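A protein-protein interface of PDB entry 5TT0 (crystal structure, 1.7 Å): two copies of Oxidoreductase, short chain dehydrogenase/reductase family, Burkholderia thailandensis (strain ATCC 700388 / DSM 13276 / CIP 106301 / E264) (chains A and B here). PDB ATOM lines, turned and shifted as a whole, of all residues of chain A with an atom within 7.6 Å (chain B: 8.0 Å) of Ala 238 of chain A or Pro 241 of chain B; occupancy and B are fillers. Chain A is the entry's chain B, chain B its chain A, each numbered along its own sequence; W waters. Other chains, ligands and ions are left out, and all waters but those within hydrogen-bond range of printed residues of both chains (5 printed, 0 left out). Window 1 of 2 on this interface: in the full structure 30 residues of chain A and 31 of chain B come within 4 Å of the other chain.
N of Asp 243 of chain B sits at hydrogen-bond distance from O of Ala 234 of chain A (3.3 Å).
The backbone NH (N) of Gly 244 of chain B is in hydrogen-bond range of the backbone carbonyl oxygen (O) of Ala 234 of chain A (2.8 Å).
Ala 238 of chain A touches Pro 241 of chain B, and with the chains exchanged Pro 241 of chain A touches Ala 238 of chain B.
Positions printed for both chains: 180, 181, 182, 227, 238, 239, 240 and 241.
N of Val 180 of chain B lies within hydrogen-bond range of O of Ala 238 of chain B.
The backbone NH (N) of Gly 184 of chain B sits at hydrogen-bond distance from the backbone carbonyl oxygen (O) of Val 242 of chain B, at 3.2 Å.
The backbone NH (N) of Leu 246 of chain B is in hydrogen-bond range of the side-chain carboxylate (OD2) of Asp 243 of chain B (3.3 Å).
The side-chain amide oxygen of Asn 179 of chain A lies close to the backbone NH of Thr 236 of chain A (3.5 Å).
Of the 22 printed residues of chain A, 7 touch a printed residue of chain B.
Printed residues of chain A that touch a printed residue of chain B: Lys 165, Phe 226, Ala 234, Ile 235, Thr 236, Ala 238 and Pro 241.
Of the 23 printed residues of chain B, 9 touch a printed residue of chain A.
Printed residues of chain B that touch a printed residue of chain A: Ala 215, Ala 223, Ala 238, Pro 241, Val 242, Asp 243, Gly 244, Gly 245 and Ala 248.
Hydrophobic or aromatic side chains of chain B that line the printed part of chain A: Ala 215, Ala 238 and Pro 241.
Among the printed residues, 11 pairs touch across the chains.
Among the printed residues, no Asp or Glu carboxylate lies within 4 Å of a Lys or Arg side-chain nitrogen of the other chain.
Water W5 lies within hydrogen-bond range of O of Met 239 of chain B (2.7 Å) and O of Met 239 of chain A (2.7 Å).
Water W2 bridges the backbone carbonyl oxygen (O) of Gly 237 of chain A and the backbone NH (N) of Ala 248 of chain B.
Water W1 lies within hydrogen-bond range of O of Thr 236 of chain A, OD2 of Asp 243 of chain B, N of Ala 248 of chain B and N of Leu 247 of chain B.
Among the printed residues, pairs that only touch across the chains: Thr 236 of chain A with Gly 245 of chain B (3.3 Å), Ile 235 of chain A with Pro 241 of chain B (3.7 Å), Ala 238 of chain A with Pro 241 of chain B (3.7 Å), Lys 165 of chain A with Ala 248 of chain B (3.8 Å), Pro 241 of chain A with Ala 238 of chain B (3.8 Å), Thr 236 of chain A with Gly 244 of chain B (3.8 Å), Ala 234 of chain A with Ala 215 of chain B (3.8 Å), Phe 226 of chain A with Ala 223 of chain B (3.97 Å) and Ala 234 of chain A with Val 242 of chain B (3.98 Å).
Of the printed residues of chain B, Ala 234 of chain A touches Ala 215 (3.8 Å), Val 242 (3.98 Å), Asp 243 (3.3 Å) and Gly 244 (2.8 Å).
Ala 238 of chain A touches just one residue of chain B: Pro 241 (3.7 Å).
Printed residues of chain A within 4 Å of Gly 245 of chain B: Thr 236.
The nearest residue of chain A that does not touch Pro 241 of chain B is Ala 234 of chain A (5.0 Å).
The nearest printed residue of chain A that does not touch Val 242 of chain B is Ile 235 of chain A (4.1 Å).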
ATOM      1  N   ILE A 136      15.054  -0.527  -1.475  1.00  0.00           N
ATOM      2  CA  ILE A 136      13.869  -1.313  -1.791  1.00  0.00           C
ATOM      3  C   ILE A 136      12.896  -1.125  -0.642  1.00  0.00           C
ATOM      4  O   ILE A 136      13.207  -1.460   0.505  1.00  0.00           O
ATOM      5  CB  ILE A 136      14.223  -2.794  -1.990  1.00  0.00           C
ATOM      6  CG1 ILE A 136      15.155  -2.950  -3.197  1.00  0.00           C
ATOM      7  CG2 ILE A 136      12.959  -3.636  -2.169  1.00  0.00           C
ATOM      8  CD1 ILE A 136      15.837  -4.313  -3.243  1.00  0.00           C
ATOM      9  N   ILE A 138       9.111  -2.033   0.478  1.00  0.00           N
ATOM     10  CA  ILE A 138       8.014  -2.938   0.148  1.00  0.00           C
ATOM     11  C   ILE A 138       6.782  -2.498   0.924  1.00  0.00           C
ATOM     12  O   ILE A 138       6.867  -2.253   2.132  1.00  0.00           O
ATOM     13  CB  ILE A 138       8.403  -4.387   0.484  1.00  0.00           C
ATOM     14  CG1 ILE A 138       9.556  -4.831  -0.432  1.00  0.00           C
ATOM     15  CG2 ILE A 138       7.199  -5.328   0.396  1.00  0.00           C
ATOM     16  CD1 ILE A 138      10.262  -6.120   0.055  1.00  0.00           C
ATOM     17  N   ILE A 161       8.032  -9.745   4.557  1.00  0.00           N
ATOM     18  CA  ILE A 161       8.886  -9.342   5.667  1.00  0.00           C
ATOM     19  C   ILE A 161      10.136 -10.206   5.703  1.00  0.00           C
ATOM     20  O   ILE A 161      11.246  -9.697   5.877  1.00  0.00           O
ATOM     21  CB  ILE A 161       8.098  -9.397   6.987  1.00  0.00           C
ATOM     22  CG1 ILE A 161       7.014  -8.312   6.974  1.00  0.00           C
ATOM     23  CG2 ILE A 161       9.040  -9.256   8.180  1.00  0.00           C
ATOM     24  CD1 ILE A 161       5.965  -8.444   8.083  1.00  0.00           C
ATOM     25  N   ALA A 164      12.417  -9.156   2.732  1.00  0.00           N
ATOM     26  CA  ALA A 164      13.157  -7.926   2.993  1.00  0.00           C
ATOM     27  C   ALA A 164      14.369  -8.194   3.876  1.00  0.00           C
ATOM     28  O   ALA A 164      15.445  -7.629   3.657  1.00  0.00           O
ATOM     29  CB  ALA A 164      12.245  -6.886   3.647  1.00  0.00           C
ATOM     30  N   LYS A 165      14.213  -9.042   4.890  1.00  0.00           N
ATOM     31  CA  LYS A 165      15.341  -9.351   5.762  1.00  0.00           C
ATOM     32  C   LYS A 165      16.416 -10.133   5.016  1.00  0.00           C
ATOM     33  O   LYS A 165      17.614  -9.895   5.207  1.00  0.00           O
ATOM     34  CB  LYS A 165      14.846 -10.121   6.991  1.00  0.00           C
ATOM     35  CG  LYS A 165      13.987  -9.251   7.895  1.00  0.00           C
ATOM     36  CD  LYS A 165      13.420 -10.004   9.080  1.00  0.00           C
ATOM     37  CE  LYS A 165      12.650  -9.034   9.962  1.00  0.00           C
ATOM     38  NZ  LYS A 165      12.096  -9.693  11.171  1.00  0.00           N
ATOM     39  N   ALA A 168      18.178  -7.625   2.936  1.00  0.00           N
ATOM     40  CA  ALA A 168      19.021  -6.761   3.753  1.00  0.00           C
ATOM     41  C   ALA A 168      20.362  -7.418   4.057  1.00  0.00           C
ATOM     42  O   ALA A 168      21.418  -6.789   3.909  1.00  0.00           O
ATOM     43  CB  ALA A 168      18.294  -6.399   5.052  1.00  0.00           C
ATOM     44  N   ALA A 178      16.677  -2.677   2.237  1.00  0.00           N
ATOM     45  CA  ALA A 178      15.347  -3.235   2.002  1.00  0.00           C
ATOM     46  C   ALA A 178      14.521  -3.153   3.277  1.00  0.00           C
ATOM     47  O   ALA A 178      14.948  -3.668   4.313  1.00  0.00           O
ATOM     48  CB  ALA A 178      15.420  -4.703   1.540  1.00  0.00           C
ATOM     49  N   ASN A 179      13.329  -2.555   3.189  1.00  0.00           N
ATOM     50  CA  ASN A 179      12.459  -2.382   4.351  1.00  0.00           C
ATOM     51  C   ASN A 179      11.004  -2.562   3.949  1.00  0.00           C
ATOM     52  O   ASN A 179      10.650  -2.499   2.771  1.00  0.00           O
ATOM     53  CB  ASN A 179      12.618  -0.992   4.986  1.00  0.00           C
ATOM     54  CG  ASN A 179      14.020  -0.743   5.494  1.00  0.00           C
ATOM     55  OD1 ASN A 179      14.415  -1.307   6.501  1.00  0.00           O
ATOM     56  ND2 ASN A 179      14.779   0.098   4.788  1.00  0.00           N
ATOM     57  N   VAL A 180      10.146  -2.738   4.949  1.00  0.00           N
ATOM     58  CA  VAL A 180       8.726  -2.976   4.710  1.00  0.00           C
ATOM     59  C   VAL A 180       7.913  -1.945   5.482  1.00  0.00           C
ATOM     60  O   VAL A 180       8.134  -1.744   6.681  1.00  0.00           O
ATOM     61  CB  VAL A 180       8.293  -4.399   5.120  1.00  0.00           C
ATOM     62  CG1 VAL A 180       6.816  -4.603   4.806  1.00  0.00           C
ATOM     63  CG2 VAL A 180       9.116  -5.457   4.394  1.00  0.00           C
ATOM     64  N   VAL A 181       6.978  -1.302   4.790  1.00  0.00           N
ATOM     65  CA  VAL A 181       5.930  -0.489   5.397  1.00  0.00           C
ATOM     66  C   VAL A 181       4.671  -1.341   5.476  1.00  0.00           C
ATOM     67  O   VAL A 181       4.264  -1.934   4.472  1.00  0.00           O
ATOM     68  CB  VAL A 181       5.675   0.779   4.569  1.00  0.00           C
ATOM     69  CG1 VAL A 181       4.462   1.520   5.091  1.00  0.00           C
ATOM     70  CG2 VAL A 181       6.888   1.683   4.601  1.00  0.00           C
ATOM     71  N   CYS A 182       4.059  -1.423   6.661  1.00  0.00           N
ATOM     72  CA  CYS A 182       2.858  -2.245   6.848  1.00  0.00           C
ATOM     73  C   CYS A 182       1.641  -1.400   7.201  1.00  0.00           C
ATOM     74  O   CYS A 182       1.412  -1.112   8.389  1.00  0.00           O
ATOM     75  CB  CYS A 182       3.090  -3.295   7.937  1.00  0.00           C
ATOM     76  SG  CYS A 182       4.274  -4.547   7.437  1.00  0.00           S
ATOM     77  N   PHE A 226      10.361   8.345   3.657  1.00  0.00           N
ATOM     78  CA  PHE A 226      11.385   8.353   4.694  1.00  0.00           C
ATOM     79  C   PHE A 226      12.313   7.152   4.551  1.00  0.00           C
ATOM     80  O   PHE A 226      13.540   7.306   4.501  1.00  0.00           O
ATOM     81  CB  PHE A 226      10.749   8.365   6.087  1.00  0.00           C
ATOM     82  CG  PHE A 226      11.734   8.068   7.178  1.00  0.00           C
ATOM     83  CD1 PHE A 226      12.700   8.995   7.527  1.00  0.00           C
ATOM     84  CD2 PHE A 226      11.730   6.833   7.815  1.00  0.00           C
ATOM     85  CE1 PHE A 226      13.628   8.711   8.539  1.00  0.00           C
ATOM     86  CE2 PHE A 226      12.656   6.544   8.810  1.00  0.00           C
ATOM     87  CZ  PHE A 226      13.595   7.479   9.173  1.00  0.00           C
ATOM     88  N   LEU A 227      11.741   5.940   4.475  1.00  0.00           N
ATOM     89  CA  LEU A 227      12.573   4.742   4.445  1.00  0.00           C
ATOM     90  C   LEU A 227      13.447   4.689   3.202  1.00  0.00           C
ATOM     91  O   LEU A 227      14.522   4.081   3.231  1.00  0.00           O
ATOM     92  CB  LEU A 227      11.703   3.489   4.520  1.00  0.00           C
ATOM     93  CG  LEU A 227      11.068   3.296   5.888  1.00  0.00           C
ATOM     94  CD1 LEU A 227      10.102   2.118   5.816  1.00  0.00           C
ATOM     95  CD2 LEU A 227      12.158   3.044   6.916  1.00  0.00           C
ATOM     96  N   ALA A 232      17.239   7.627   6.386  1.00  0.00           N
ATOM     97  CA  ALA A 232      17.090   6.250   6.838  1.00  0.00           C
ATOM     98  C   ALA A 232      18.250   5.398   6.335  1.00  0.00           C
ATOM     99  O   ALA A 232      18.096   4.194   6.127  1.00  0.00           O
ATOM    100  CB  ALA A 232      15.761   5.665   6.363  1.00  0.00           C
ATOM    101  N   ALA A 234      20.740   4.155   7.660  1.00  0.00           N
ATOM    102  CA  ALA A 234      21.154   3.068   8.534  1.00  0.00           C
ATOM    103  C   ALA A 234      20.022   2.089   8.825  1.00  0.00           C
ATOM    104  O   ALA A 234      20.161   1.231   9.701  1.00  0.00           O
ATOM    105  CB  ALA A 234      21.725   3.631   9.841  1.00  0.00           C
ATOM    106  N   ILE A 235      18.908   2.188   8.106  1.00  0.00           N
ATOM    107  CA  ILE A 235      17.735   1.368   8.374  1.00  0.00           C
ATOM    108  C   ILE A 235      17.602   0.338   7.261  1.00  0.00           C
ATOM    109  O   ILE A 235      17.410   0.694   6.094  1.00  0.00           O
ATOM    110  CB  ILE A 235      16.460   2.217   8.489  1.00  0.00           C
ATOM    111  CG1 ILE A 235      16.639   3.271   9.600  1.00  0.00           C
ATOM    112  CG2 ILE A 235      15.258   1.307   8.756  1.00  0.00           C
ATOM    113  CD1 ILE A 235      15.402   4.143   9.832  1.00  0.00           C
ATOM    114  N   THR A 236      17.694  -0.939   7.620  1.00  0.00           N
ATOM    115  CA  THR A 236      17.471  -1.981   6.635  1.00  0.00           C
ATOM    116  C   THR A 236      16.979  -3.227   7.360  1.00  0.00           C
ATOM    117  O   THR A 236      17.363  -3.495   8.506  1.00  0.00           O
ATOM    118  CB  THR A 236      18.733  -2.248   5.797  1.00  0.00           C
ATOM    119  OG1 THR A 236      18.412  -3.083   4.683  1.00  0.00           O
ATOM    120  CG2 THR A 236      19.820  -2.931   6.613  1.00  0.00           C
ATOM    121  N   GLY A 237      16.081  -3.955   6.699  1.00  0.00           N
ATOM    122  CA  GLY A 237      15.476  -5.114   7.305  1.00  0.00           C
ATOM    123  C   GLY A 237      14.351  -4.794   8.261  1.00  0.00           C
ATOM    124  O   GLY A 237      13.900  -5.691   8.990  1.00  0.00           O
ATOM    125  N   ALA A 238      13.886  -3.550   8.280  1.00  0.00           N
ATOM    126  CA  ALA A 238      12.931  -3.106   9.280  1.00  0.00           C
ATOM    127  C   ALA A 238      11.509  -3.258   8.768  1.00  0.00           C
ATOM    128  O   ALA A 238      11.246  -3.192   7.565  1.00  0.00           O
ATOM    129  CB  ALA A 238      13.193  -1.648   9.667  1.00  0.00           C
ATOM    130  N   MET A 239      10.593  -3.457   9.707  1.00  0.00           N
ATOM    131  CA  MET A 239       9.157  -3.485   9.449  1.00  0.00           C
ATOM    132  C   MET A 239       8.553  -2.286  10.172  1.00  0.00           C
ATOM    133  O   MET A 239       8.577  -2.231  11.405  1.00  0.00           O
ATOM    134  CB  MET A 239       8.558  -4.805   9.945  1.00  0.00           C
ATOM    135  CG  MET A 239       7.085  -5.065   9.607  1.00  0.00           C
ATOM    136  SD  MET A 239       5.858  -4.128  10.545  1.00  0.00           S
ATOM    137  CE  MET A 239       5.979  -4.791  12.204  1.00  0.00           C
ATOM    138  N   LEU A 240       8.015  -1.331   9.410  1.00  0.00           N
ATOM    139  CA  LEU A 240       7.443  -0.125   9.998  1.00  0.00           C
ATOM    140  C   LEU A 240       5.926  -0.110   9.833  1.00  0.00           C
ATOM    141  O   LEU A 240       5.436   0.084   8.708  1.00  0.00           O
ATOM    142  CB  LEU A 240       8.060   1.118   9.356  1.00  0.00           C
ATOM    143  CG  LEU A 240       7.547   2.488   9.793  1.00  0.00           C
ATOM    144  CD1 LEU A 240       7.752   2.685  11.303  1.00  0.00           C
ATOM    145  CD2 LEU A 240       8.276   3.579   9.009  1.00  0.00           C
ATOM    146  N   PRO A 241       5.144  -0.278  10.904  1.00  0.00           N
ATOM    147  CA  PRO A 241       3.680  -0.229  10.763  1.00  0.00           C
ATOM    148  C   PRO A 241       3.194   1.204  10.607  1.00  0.00           C
ATOM    149  O   PRO A 241       3.629   2.098  11.336  1.00  0.00           O
ATOM    150  CB  PRO A 241       3.167  -0.842  12.073  1.00  0.00           C
ATOM    151  CG  PRO A 241       4.389  -1.337  12.823  1.00  0.00           C
ATOM    152  CD  PRO A 241       5.554  -0.556  12.288  1.00  0.00           C
ATOM    153  N   SER B 141      16.816   0.158  22.281  1.00  0.00           N
ATOM    154  CA  SER B 141      18.041  -0.515  21.884  1.00  0.00           C
ATOM    155  C   SER B 141      17.669  -1.820  21.210  1.00  0.00           C
ATOM    156  O   SER B 141      16.660  -2.439  21.563  1.00  0.00           O
ATOM    157  CB  SER B 141      18.944  -0.802  23.086  1.00  0.00           C
ATOM    158  OG  SER B 141      20.045  -1.610  22.698  1.00  0.00           O
ATOM    159  N   VAL B 142      18.497  -2.236  20.246  1.00  0.00           N
ATOM    160  CA  VAL B 142      18.334  -3.568  19.678  1.00  0.00           C
ATOM    161  C   VAL B 142      18.464  -4.629  20.767  1.00  0.00           C
ATOM    162  O   VAL B 142      17.937  -5.733  20.611  1.00  0.00           O
ATOM    163  CB  VAL B 142      19.337  -3.826  18.523  1.00  0.00           C
ATOM    164  CG1 VAL B 142      19.070  -2.880  17.334  1.00  0.00           C
ATOM    165  CG2 VAL B 142      20.782  -3.709  18.994  1.00  0.00           C
ATOM    166  N   VAL B 145      15.376  -6.412  22.022  1.00  0.00           N
ATOM    167  CA  VAL B 145      14.693  -7.304  21.098  1.00  0.00           C
ATOM    168  C   VAL B 145      15.425  -8.636  20.990  1.00  0.00           C
ATOM    169  O   VAL B 145      14.798  -9.681  20.780  1.00  0.00           O
ATOM    170  CB  VAL B 145      14.569  -6.642  19.707  1.00  0.00           C
ATOM    171  CG1 VAL B 145      13.853  -7.561  18.732  1.00  0.00           C
ATOM    172  CG2 VAL B 145      13.838  -5.320  19.826  1.00  0.00           C
ATOM    173  N   VAL B 180       9.189   3.723  19.566  1.00  0.00           N
ATOM    174  CA  VAL B 180      10.541   3.418  20.034  1.00  0.00           C
ATOM    175  C   VAL B 180      11.491   3.347  18.843  1.00  0.00           C
ATOM    176  O   VAL B 180      11.235   2.617  17.877  1.00  0.00           O
ATOM    177  CB  VAL B 180      10.590   2.090  20.814  1.00  0.00           C
ATOM    178  CG1 VAL B 180      12.002   1.834  21.331  1.00  0.00           C
ATOM    179  CG2 VAL B 180       9.614   2.102  21.978  1.00  0.00           C
ATOM    180  N   VAL B 181      12.583   4.105  18.916  1.00  0.00           N
ATOM    181  CA  VAL B 181      13.720   3.950  18.013  1.00  0.00           C
ATOM    182  C   VAL B 181      14.742   3.059  18.696  1.00  0.00           C
ATOM    183  O   VAL B 181      15.152   3.350  19.823  1.00  0.00           O
ATOM    184  CB  VAL B 181      14.355   5.306  17.669  1.00  0.00           C
ATOM    185  CG1 VAL B 181      15.624   5.089  16.864  1.00  0.00           C
ATOM    186  CG2 VAL B 181      13.385   6.156  16.898  1.00  0.00           C
ATOM    187  N   CYS B 182      15.180   1.992  18.008  1.00  0.00           N
ATOM    188  CA  CYS B 182      16.088   0.995  18.580  1.00  0.00           C
ATOM    189  C   CYS B 182      17.437   1.007  17.878  1.00  0.00           C
ATOM    190  O   CYS B 182      17.627   0.317  16.861  1.00  0.00           O
ATOM    191  CB  CYS B 182      15.463  -0.403  18.522  1.00  0.00           C
ATOM    192  SG  CYS B 182      14.148  -0.585  19.731  1.00  0.00           S
ATOM    193  N   PRO B 183      18.407   1.765  18.380  1.00  0.00           N
ATOM    194  CA  PRO B 183      19.727   1.785  17.756  1.00  0.00           C
ATOM    195  C   PRO B 183      20.476   0.491  17.995  1.00  0.00           C
ATOM    196  O   PRO B 183      20.328  -0.157  19.037  1.00  0.00           O
ATOM    197  CB  PRO B 183      20.445   2.949  18.456  1.00  0.00           C
ATOM    198  CG  PRO B 183      19.373   3.684  19.217  1.00  0.00           C
ATOM    199  CD  PRO B 183      18.331   2.670  19.538  1.00  0.00           C
ATOM    200  N   GLY B 184      21.324   0.152  17.020  1.00  0.00           N
ATOM    201  CA  GLY B 184      22.379  -0.823  17.218  1.00  0.00           C
ATOM    202  C   GLY B 184      23.588  -0.148  17.829  1.00  0.00           C
ATOM    203  O   GLY B 184      23.472   0.840  18.563  1.00  0.00           O
ATOM    204  N   ALA B 215      25.154   2.707  12.569  1.00  0.00           N
ATOM    205  CA  ALA B 215      24.406   3.947  12.665  1.00  0.00           C
ATOM    206  C   ALA B 215      25.238   4.975  13.417  1.00  0.00           C
ATOM    207  O   ALA B 215      26.007   4.642  14.325  1.00  0.00           O
ATOM    208  CB  ALA B 215      23.071   3.721  13.375  1.00  0.00           C
ATOM    209  N   VAL B 220      20.363   8.121  14.209  1.00  0.00           N
ATOM    210  CA  VAL B 220      19.345   7.930  15.232  1.00  0.00           C
ATOM    211  C   VAL B 220      18.470   9.167  15.364  1.00  0.00           C
ATOM    212  O   VAL B 220      17.238   9.069  15.432  1.00  0.00           O
ATOM    213  CB  VAL B 220      20.009   7.562  16.570  1.00  0.00           C
ATOM    214  CG1 VAL B 220      18.947   7.422  17.659  1.00  0.00           C
ATOM    215  CG2 VAL B 220      20.823   6.273  16.387  1.00  0.00           C
ATOM    216  N   ALA B 223      15.806   9.424  12.634  1.00  0.00           N
ATOM    217  CA  ALA B 223      14.645   8.570  12.845  1.00  0.00           C
ATOM    218  C   ALA B 223      13.737   9.139  13.930  1.00  0.00           C
ATOM    219  O   ALA B 223      12.505   9.097  13.809  1.00  0.00           O
ATOM    220  CB  ALA B 223      15.091   7.150  13.213  1.00  0.00           C
ATOM    221  N   LEU B 227       9.793  10.179  13.448  1.00  0.00           N
ATOM    222  CA  LEU B 227       8.700   9.618  14.232  1.00  0.00           C
ATOM    223  C   LEU B 227       7.987  10.684  15.036  1.00  0.00           C
ATOM    224  O   LEU B 227       6.814  10.514  15.362  1.00  0.00           O
ATOM    225  CB  LEU B 227       9.216   8.527  15.168  1.00  0.00           C
ATOM    226  CG  LEU B 227       9.626   7.250  14.447  1.00  0.00           C
ATOM    227  CD1 LEU B 227      10.264   6.308  15.440  1.00  0.00           C
ATOM    228  CD2 LEU B 227       8.405   6.598  13.784  1.00  0.00           C
ATOM    229  N   ALA B 238       5.079   1.709  17.380  1.00  0.00           N
ATOM    230  CA  ALA B 238       6.024   1.065  16.485  1.00  0.00           C
ATOM    231  C   ALA B 238       7.403   0.983  17.121  1.00  0.00           C
ATOM    232  O   ALA B 238       7.787   1.827  17.935  1.00  0.00           O
ATOM    233  CB  ALA B 238       6.122   1.815  15.155  1.00  0.00           C
ATOM    234  N   MET B 239       8.135  -0.057  16.736  1.00  0.00           N
ATOM    235  CA  MET B 239       9.543  -0.223  17.070  1.00  0.00           C
ATOM    236  C   MET B 239      10.322  -0.121  15.766  1.00  0.00           C
ATOM    237  O   MET B 239      10.149  -0.958  14.872  1.00  0.00           O
ATOM    238  CB  MET B 239       9.776  -1.575  17.756  1.00  0.00           C
ATOM    239  CG  MET B 239      11.180  -1.832  18.304  1.00  0.00           C
ATOM    240  SD  MET B 239      12.450  -2.238  17.072  1.00  0.00           S
ATOM    241  CE  MET B 239      11.912  -3.811  16.402  1.00  0.00           C
ATOM    242  N   LEU B 240      11.160   0.902  15.654  1.00  0.00           N
ATOM    243  CA  LEU B 240      11.936   1.123  14.443  1.00  0.00           C
ATOM    244  C   LEU B 240      13.415   0.902  14.727  1.00  0.00           C
ATOM    245  O   LEU B 240      14.051   1.739  15.396  1.00  0.00           O
ATOM    246  CB  LEU B 240      11.700   2.538  13.915  1.00  0.00           C
ATOM    247  CG  LEU B 240      12.461   2.980  12.665  1.00  0.00           C
ATOM    248  CD1 LEU B 240      12.130   2.092  11.474  1.00  0.00           C
ATOM    249  CD2 LEU B 240      12.146   4.438  12.349  1.00  0.00           C
ATOM    250  N   PRO B 241      14.008  -0.170  14.221  1.00  0.00           N
ATOM    251  CA  PRO B 241      15.446  -0.361  14.413  1.00  0.00           C
ATOM    252  C   PRO B 241      16.249   0.567  13.518  1.00  0.00           C
ATOM    253  O   PRO B 241      15.943   0.757  12.337  1.00  0.00           O
ATOM    254  CB  PRO B 241      15.662  -1.835  14.046  1.00  0.00           C
ATOM    255  CG  PRO B 241      14.543  -2.164  13.111  1.00  0.00           C
ATOM    256  CD  PRO B 241      13.389  -1.255  13.436  1.00  0.00           C
ATOM    257  N   VAL B 242      17.283   1.164  14.110  1.00  0.00           N
ATOM    258  CA  VAL B 242      18.224   1.995  13.375  1.00  0.00           C
ATOM    259  C   VAL B 242      19.581   1.360  13.633  1.00  0.00           C
ATOM    260  O   VAL B 242      20.330   1.787  14.512  1.00  0.00           O
ATOM    261  CB  VAL B 242      18.142   3.467  13.821  1.00  0.00           C
ATOM    262  CG1 VAL B 242      19.048   4.346  12.969  1.00  0.00           C
ATOM    263  CG2 VAL B 242      16.696   3.938  13.708  1.00  0.00           C
ATOM    264  N   ASP B 243      19.875   0.286  12.891  1.00  0.00           N
ATOM    265  CA  ASP B 243      20.842  -0.679  13.392  1.00  0.00           C
ATOM    266  C   ASP B 243      21.702  -1.279  12.289  1.00  0.00           C
ATOM    267  O   ASP B 243      22.290  -2.342  12.496  1.00  0.00           O
ATOM    268  CB  ASP B 243      20.113  -1.809  14.133  1.00  0.00           C
ATOM    269  CG  ASP B 243      19.240  -2.653  13.198  1.00  0.00           C
ATOM    270  OD1 ASP B 243      19.070  -2.261  12.017  1.00  0.00           O
ATOM    271  OD2 ASP B 243      18.731  -3.702  13.645  1.00  0.00           O
ATOM    272  N   GLY B 244      21.764  -0.641  11.120  1.00  0.00           N
ATOM    273  CA  GLY B 244      22.589  -1.134  10.037  1.00  0.00           C
ATOM    274  C   GLY B 244      22.154  -2.504   9.556  1.00  0.00           C
ATOM    275  O   GLY B 244      22.904  -3.171   8.841  1.00  0.00           O
ATOM    276  N   GLY B 245      20.958  -2.935   9.957  1.00  0.00           N
ATOM    277  CA  GLY B 245      20.441  -4.241   9.595  1.00  0.00           C
ATOM    278  C   GLY B 245      20.668  -5.344  10.600  1.00  0.00           C
ATOM    279  O   GLY B 245      20.397  -6.511  10.277  1.00  0.00           O
ATOM    280  N   LEU B 246      21.123  -5.013  11.813  1.00  0.00           N
ATOM    281  CA  LEU B 246      21.533  -6.038  12.771  1.00  0.00           C
ATOM    282  C   LEU B 246      20.399  -7.002  13.103  1.00  0.00           C
ATOM    283  O   LEU B 246      20.601  -8.225  13.148  1.00  0.00           O
ATOM    284  CB  LEU B 246      22.053  -5.372  14.046  1.00  0.00           C
ATOM    285  CG  LEU B 246      22.681  -6.351  15.042  1.00  0.00           C
ATOM    286  CD1 LEU B 246      23.963  -6.896  14.430  1.00  0.00           C
ATOM    287  CD2 LEU B 246      22.951  -5.666  16.388  1.00  0.00           C
ATOM    288  N   LEU B 247      19.197  -6.483  13.342  1.00  0.00           N
ATOM    289  CA  LEU B 247      18.132  -7.369  13.799  1.00  0.00           C
ATOM    290  C   LEU B 247      17.532  -8.220  12.687  1.00  0.00           C
ATOM    291  O   LEU B 247      16.727  -9.116  12.981  1.00  0.00           O
ATOM    292  CB  LEU B 247      17.027  -6.554  14.472  1.00  0.00           C
ATOM    293  CG  LEU B 247      17.348  -5.977  15.846  1.00  0.00           C
ATOM    294  CD1 LEU B 247      16.190  -5.070  16.282  1.00  0.00           C
ATOM    295  CD2 LEU B 247      17.590  -7.091  16.870  1.00  0.00           C
ATOM    296  N   ALA B 248      17.922  -7.999  11.433  1.00  0.00           N
ATOM    297  CA  ALA B 248      17.316  -8.765  10.346  1.00  0.00           C
ATOM    298  C   ALA B 248      17.690 -10.239  10.412  1.00  0.00           C
ATOM    299  O   ALA B 248      16.921 -11.095   9.964  1.00  0.00           O
ATOM    300  CB  ALA B 248      17.721  -8.186   8.992  1.00  0.00           C
HETATM  301  O   HOH W   1      17.259  -4.665  11.118  1.00  0.00           O
HETATM  302  O   HOH W   2      15.007  -6.198  11.447  1.00  0.00           O
HETATM  303  O   HOH W   3      17.195  -1.127  10.574  1.00  0.00           O
HETATM  304  O   HOH W   4      14.607 -11.150  12.364  1.00  0.00           O
HETATM  305  O   HOH W   5       9.107  -3.269  13.876  1.00  0.00           O
